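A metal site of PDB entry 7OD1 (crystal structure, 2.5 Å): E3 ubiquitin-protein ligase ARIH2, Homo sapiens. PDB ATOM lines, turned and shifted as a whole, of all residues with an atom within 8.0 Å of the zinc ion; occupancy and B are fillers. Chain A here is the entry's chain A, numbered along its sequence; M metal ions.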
ATOM      1  N   ASN A 311      21.912  -6.563   0.562  1.00  0.00           N
ATOM      2  CA  ASN A 311      21.841  -6.537  -0.890  1.00  0.00           C
ATOM      3  C   ASN A 311      21.863  -7.920  -1.515  1.00  0.00           C
ATOM      4  O   ASN A 311      21.815  -8.027  -2.742  1.00  0.00           O
ATOM      5  CB  ASN A 311      22.982  -5.684  -1.448  1.00  0.00           C
ATOM      6  CG  ASN A 311      22.878  -4.229  -1.033  1.00  0.00           C
ATOM      7  OD1 ASN A 311      21.909  -3.540  -1.343  1.00  0.00           O
ATOM      8  ND2 ASN A 311      23.887  -3.749  -0.311  1.00  0.00           N
ATOM      9  N   PHE A 322      20.526 -13.313  -5.947  1.00  0.00           N
ATOM     10  CA  PHE A 322      21.176 -12.308  -6.768  1.00  0.00           C
ATOM     11  C   PHE A 322      21.595 -11.119  -5.922  1.00  0.00           C
ATOM     12  O   PHE A 322      21.333 -11.057  -4.717  1.00  0.00           O
ATOM     13  CB  PHE A 322      20.292 -11.871  -7.946  1.00  0.00           C
ATOM     14  CG  PHE A 322      18.972 -11.267  -7.533  1.00  0.00           C
ATOM     15  CD1 PHE A 322      17.917 -12.075  -7.153  1.00  0.00           C
ATOM     16  CD2 PHE A 322      18.785  -9.893  -7.570  1.00  0.00           C
ATOM     17  CE1 PHE A 322      16.698 -11.530  -6.779  1.00  0.00           C
ATOM     18  CE2 PHE A 322      17.568  -9.338  -7.195  1.00  0.00           C
ATOM     19  CZ  PHE A 322      16.529 -10.162  -6.805  1.00  0.00           C
ATOM     20  N   CYS A 323      22.261 -10.164  -6.566  1.00  0.00           N
ATOM     21  CA  CYS A 323      22.789  -8.971  -5.932  1.00  0.00           C
ATOM     22  C   CYS A 323      21.964  -7.760  -6.362  1.00  0.00           C
ATOM     23  O   CYS A 323      21.660  -7.602  -7.543  1.00  0.00           O
ATOM     24  CB  CYS A 323      24.263  -8.767  -6.275  1.00  0.00           C
ATOM     25  SG  CYS A 323      24.849  -7.050  -6.148  1.00  0.00           S
ATOM     26  N   TRP A 324      21.604  -6.905  -5.393  1.00  0.00           N
ATOM     27  CA  TRP A 324      20.677  -5.811  -5.682  1.00  0.00           C
ATOM     28  C   TRP A 324      21.291  -4.774  -6.624  1.00  0.00           C
ATOM     29  O   TRP A 324      20.570  -4.124  -7.381  1.00  0.00           O
ATOM     30  CB  TRP A 324      20.215  -5.140  -4.387  1.00  0.00           C
ATOM     31  CG  TRP A 324      19.264  -3.955  -4.581  1.00  0.00           C
ATOM     32  CD1 TRP A 324      19.593  -2.637  -4.499  1.00  0.00           C
ATOM     33  CD2 TRP A 324      17.861  -4.010  -4.879  1.00  0.00           C
ATOM     34  NE1 TRP A 324      18.478  -1.852  -4.737  1.00  0.00           N
ATOM     35  CE2 TRP A 324      17.409  -2.674  -4.972  1.00  0.00           C
ATOM     36  CE3 TRP A 324      16.952  -5.045  -5.081  1.00  0.00           C
ATOM     37  CZ2 TRP A 324      16.072  -2.351  -5.250  1.00  0.00           C
ATOM     38  CZ3 TRP A 324      15.625  -4.725  -5.358  1.00  0.00           C
ATOM     39  CH2 TRP A 324      15.210  -3.401  -5.439  1.00  0.00           C
ATOM     40  N   MET A 325      22.615  -4.616  -6.593  1.00  0.00           N
ATOM     41  CA  MET A 325      23.282  -3.624  -7.425  1.00  0.00           C
ATOM     42  C   MET A 325      23.516  -4.164  -8.835  1.00  0.00           C
ATOM     43  O   MET A 325      23.391  -3.429  -9.818  1.00  0.00           O
ATOM     44  CB  MET A 325      24.617  -3.229  -6.793  1.00  0.00           C
ATOM     45  CG  MET A 325      24.491  -2.359  -5.550  1.00  0.00           C
ATOM     46  SD  MET A 325      23.582  -0.845  -5.869  1.00  0.00           S
ATOM     47  CE  MET A 325      24.662  -0.073  -7.068  1.00  0.00           C
ATOM     48  N   CYS A 326      23.853  -5.442  -8.949  1.00  0.00           N
ATOM     49  CA  CYS A 326      24.122  -6.125 -10.205  1.00  0.00           C
ATOM     50  C   CYS A 326      22.863  -6.573 -10.930  1.00  0.00           C
ATOM     51  O   CYS A 326      22.711  -6.314 -12.127  1.00  0.00           O
ATOM     52  CB  CYS A 326      24.996  -7.359  -9.987  1.00  0.00           C
ATOM     53  SG  CYS A 326      26.645  -7.036  -9.383  1.00  0.00           S
ATOM     54  N   LEU A 327      21.950  -7.222 -10.201  1.00  0.00           N
ATOM     55  CA  LEU A 327      20.977  -8.159 -10.771  1.00  0.00           C
ATOM     56  C   LEU A 327      21.688  -9.390 -11.335  1.00  0.00           C
ATOM     57  O   LEU A 327      21.183 -10.053 -12.246  1.00  0.00           O
ATOM     58  CB  LEU A 327      20.075  -7.521 -11.825  1.00  0.00           C
ATOM     59  CG  LEU A 327      19.312  -6.280 -11.357  1.00  0.00           C
ATOM     60  CD1 LEU A 327      18.346  -5.771 -12.420  1.00  0.00           C
ATOM     61  CD2 LEU A 327      18.594  -6.586 -10.050  1.00  0.00           C
ATOM     62  N   GLY A 328      22.870  -9.682 -10.803  1.00  0.00           N
ATOM     63  CA  GLY A 328      23.634 -10.859 -11.169  1.00  0.00           C
ATOM     64  C   GLY A 328      23.659 -11.853 -10.027  1.00  0.00           C
ATOM     65  O   GLY A 328      23.400 -11.476  -8.881  1.00  0.00           O
ATOM     66  N   ASP A 329      23.971 -13.112 -10.313  1.00  0.00           N
ATOM     67  CA  ASP A 329      23.746 -14.150  -9.318  1.00  0.00           C
ATOM     68  C   ASP A 329      24.725 -13.988  -8.163  1.00  0.00           C
ATOM     69  O   ASP A 329      25.806 -13.414  -8.294  1.00  0.00           O
ATOM     70  CB  ASP A 329      23.902 -15.537  -9.939  1.00  0.00           C
ATOM     71  CG  ASP A 329      23.438 -16.639  -9.012  1.00  0.00           C
ATOM     72  OD1 ASP A 329      23.995 -16.795  -7.895  1.00  0.00           O
ATOM     73  OD2 ASP A 329      22.498 -17.360  -9.389  1.00  0.00           O
ATOM     74  N   TRP A 330      24.314 -14.510  -7.000  1.00  0.00           N
ATOM     75  CA  TRP A 330      25.068 -14.317  -5.772  1.00  0.00           C
ATOM     76  C   TRP A 330      26.251 -15.266  -5.636  1.00  0.00           C
ATOM     77  O   TRP A 330      27.128 -14.984  -4.808  1.00  0.00           O
ATOM     78  CB  TRP A 330      24.142 -14.458  -4.563  1.00  0.00           C
ATOM     79  CG  TRP A 330      24.779 -13.950  -3.296  1.00  0.00           C
ATOM     80  CD1 TRP A 330      25.229 -14.694  -2.248  1.00  0.00           C
ATOM     81  CD2 TRP A 330      25.042 -12.581  -2.957  1.00  0.00           C
ATOM     82  NE1 TRP A 330      25.748 -13.880  -1.270  1.00  0.00           N
ATOM     83  CE2 TRP A 330      25.650 -12.580  -1.686  1.00  0.00           C
ATOM     84  CE3 TRP A 330      24.814 -11.361  -3.606  1.00  0.00           C
ATOM     85  CZ2 TRP A 330      26.040 -11.396  -1.048  1.00  0.00           C
ATOM     86  CZ3 TRP A 330      25.200 -10.196  -2.971  1.00  0.00           C
ATOM     87  CH2 TRP A 330      25.811 -10.226  -1.705  1.00  0.00           C
ATOM     88  N   THR A 332      28.682 -15.531  -7.378  1.00  0.00           N
ATOM     89  CA  THR A 332      29.847 -14.727  -7.716  1.00  0.00           C
ATOM     90  C   THR A 332      30.171 -13.691  -6.662  1.00  0.00           C
ATOM     91  O   THR A 332      31.187 -13.000  -6.770  1.00  0.00           O
ATOM     92  CB  THR A 332      29.628 -14.006  -9.048  1.00  0.00           C
ATOM     93  OG1 THR A 332      28.351 -13.338  -9.018  1.00  0.00           O
ATOM     94  CG2 THR A 332      29.656 -14.994 -10.209  1.00  0.00           C
ATOM     95  N   HIS A 333      29.322 -13.543  -5.640  1.00  0.00           N
ATOM     96  CA  HIS A 333      29.469 -12.519  -4.617  1.00  0.00           C
ATOM     97  C   HIS A 333      29.825 -13.143  -3.264  1.00  0.00           C
ATOM     98  O   HIS A 333      29.363 -12.697  -2.211  1.00  0.00           O
ATOM     99  CB  HIS A 333      28.212 -11.672  -4.514  1.00  0.00           C
ATOM    100  CG  HIS A 333      28.080 -10.627  -5.568  1.00  0.00           C
ATOM    101  ND1 HIS A 333      28.203 -10.900  -6.916  1.00  0.00           N
ATOM    102  CD2 HIS A 333      27.798  -9.305  -5.482  1.00  0.00           C
ATOM    103  CE1 HIS A 333      28.021  -9.797  -7.609  1.00  0.00           C
ATOM    104  NE2 HIS A 333      27.776  -8.809  -6.768  1.00  0.00           N
ATOM    105  N   TYR A 338      35.508 -11.461  -4.831  1.00  0.00           N
ATOM    106  CA  TYR A 338      34.456 -10.448  -4.810  1.00  0.00           C
ATOM    107  C   TYR A 338      34.813  -9.339  -5.799  1.00  0.00           C
ATOM    108  O   TYR A 338      35.831  -8.649  -5.633  1.00  0.00           O
ATOM    109  CB  TYR A 338      34.262  -9.875  -3.410  1.00  0.00           C
ATOM    110  CG  TYR A 338      32.961  -9.115  -3.286  1.00  0.00           C
ATOM    111  CD1 TYR A 338      31.767  -9.772  -3.018  1.00  0.00           C
ATOM    112  CD2 TYR A 338      32.919  -7.731  -3.448  1.00  0.00           C
ATOM    113  CE1 TYR A 338      30.571  -9.087  -2.914  1.00  0.00           C
ATOM    114  CE2 TYR A 338      31.726  -7.036  -3.342  1.00  0.00           C
ATOM    115  CZ  TYR A 338      30.559  -7.710  -3.074  1.00  0.00           C
ATOM    116  OH  TYR A 338      29.375  -7.018  -2.968  1.00  0.00           O
ATOM    117  N   GLU A 339      33.972  -9.173  -6.824  1.00  0.00           N
ATOM    118  CA  GLU A 339      34.249  -8.235  -7.902  1.00  0.00           C
ATOM    119  C   GLU A 339      33.289  -7.046  -7.943  1.00  0.00           C
ATOM    120  O   GLU A 339      33.615  -6.039  -8.576  1.00  0.00           O
ATOM    121  CB  GLU A 339      34.172  -8.960  -9.255  1.00  0.00           C
ATOM    122  CG  GLU A 339      35.246 -10.027  -9.506  1.00  0.00           C
ATOM    123  CD  GLU A 339      36.670  -9.583  -9.244  1.00  0.00           C
ATOM    124  OE1 GLU A 339      37.513 -10.439  -8.935  1.00  0.00           O
ATOM    125  OE2 GLU A 339      36.964  -8.378  -9.398  1.00  0.00           O
ATOM    126  N   CYS A 340      32.131  -7.140  -7.271  1.00  0.00           N
ATOM    127  CA  CYS A 340      31.061  -6.168  -7.453  1.00  0.00           C
ATOM    128  C   CYS A 340      31.488  -4.753  -7.078  1.00  0.00           C
ATOM    129  O   CYS A 340      30.975  -3.772  -7.645  1.00  0.00           O
ATOM    130  CB  CYS A 340      29.830  -6.587  -6.640  1.00  0.00           C
ATOM    131  SG  CYS A 340      28.481  -5.374  -6.516  1.00  0.00           S
ATOM    132  N   SER A 341      32.428  -4.602  -6.143  1.00  0.00           N
ATOM    133  CA  SER A 341      32.766  -3.289  -5.612  1.00  0.00           C
ATOM    134  C   SER A 341      33.830  -2.558  -6.422  1.00  0.00           C
ATOM    135  O   SER A 341      33.936  -1.329  -6.298  1.00  0.00           O
ATOM    136  CB  SER A 341      33.216  -3.411  -4.154  1.00  0.00           C
ATOM    137  OG  SER A 341      34.311  -4.303  -4.038  1.00  0.00           O
ATOM    138  N   PHE A 367      28.941   4.781 -11.140  1.00  0.00           N
ATOM    139  CA  PHE A 367      29.260   3.517 -10.488  1.00  0.00           C
ATOM    140  C   PHE A 367      29.546   3.724  -9.005  1.00  0.00           C
ATOM    141  O   PHE A 367      29.112   2.915  -8.168  1.00  0.00           O
ATOM    142  CB  PHE A 367      30.466   2.844 -11.160  1.00  0.00           C
ATOM    143  CG  PHE A 367      30.930   1.589 -10.471  1.00  0.00           C
ATOM    144  CD1 PHE A 367      30.395   0.363 -10.816  1.00  0.00           C
ATOM    145  CD2 PHE A 367      31.904   1.647  -9.476  1.00  0.00           C
ATOM    146  CE1 PHE A 367      30.815  -0.798 -10.177  1.00  0.00           C
ATOM    147  CE2 PHE A 367      32.326   0.496  -8.835  1.00  0.00           C
ATOM    148  CZ  PHE A 367      31.782  -0.726  -9.191  1.00  0.00           C
ATOM    149  N   ARG A 371      26.456   3.206  -5.457  1.00  0.00           N
ATOM    150  CA  ARG A 371      26.772   2.378  -4.295  1.00  0.00           C
ATOM    151  C   ARG A 371      26.788   3.205  -3.013  1.00  0.00           C
ATOM    152  O   ARG A 371      26.333   2.726  -1.961  1.00  0.00           O
ATOM    153  CB  ARG A 371      28.098   1.649  -4.503  1.00  0.00           C
ATOM    154  CG  ARG A 371      27.928   0.333  -5.231  1.00  0.00           C
ATOM    155  CD  ARG A 371      29.188  -0.075  -5.985  1.00  0.00           C
ATOM    156  NE  ARG A 371      28.937  -1.217  -6.855  1.00  0.00           N
ATOM    157  CZ  ARG A 371      28.369  -1.127  -8.056  1.00  0.00           C
ATOM    158  NH1 ARG A 371      28.004   0.038  -8.565  1.00  0.00           N
ATOM    159  NH2 ARG A 371      28.187  -2.245  -8.762  1.00  0.00           N
ATOM    160  N   GLU A 451      32.754  -5.428   2.077  1.00  0.00           N
ATOM    161  CA  GLU A 451      31.400  -5.472   1.552  1.00  0.00           C
ATOM    162  C   GLU A 451      30.832  -6.888   1.580  1.00  0.00           C
ATOM    163  O   GLU A 451      29.675  -7.100   1.936  1.00  0.00           O
ATOM    164  CB  GLU A 451      31.362  -4.915   0.132  1.00  0.00           C
ATOM    165  CG  GLU A 451      29.971  -4.849  -0.481  1.00  0.00           C
ATOM    166  CD  GLU A 451      29.868  -3.823  -1.586  1.00  0.00           C
ATOM    167  OE1 GLU A 451      30.202  -2.642  -1.343  1.00  0.00           O
ATOM    168  OE2 GLU A 451      29.453  -4.195  -2.704  1.00  0.00           O
HETATM  169 ZN    ZN M   1      26.947  -6.996  -7.109  1.00  0.00          ZN
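The guanidinium group (NE) of Arg 371 is in hydrogen-bond range of the backbone carbonyl oxygen (O) of Cys 340. SG of Cys 323 sits close to N of Met 325 (3.3 Å). A ring nitrogen (ND1) of His 333 sits at hydrogen-bond distance from the side-chain hydroxyl (OG1) of Thr 332, at 3.2 Å. The backbone NH (N) of Cys 323 lies within hydrogen-bond range of the backbone carbonyl oxygen (O) of Gly 328.
Of the 19 residues printed, 4 come within 4 Å of the zinc ion. Along chain A the residues within 4 Å of the zinc ion span positions 323 to 340. The nearest printed residue that does not touch the zinc ion is Met 325 (4.4 Å).
NE2 of His 333 binds the zinc ion, at 2.0 Å. SG of Cys 326 binds the zinc ion (2.3 Å). The zinc ion is bound by the side-chain sulfur (SG) of Cys 323, 2.3 Å away. SG of Cys 340 binds the zinc ion (2.3 Å).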
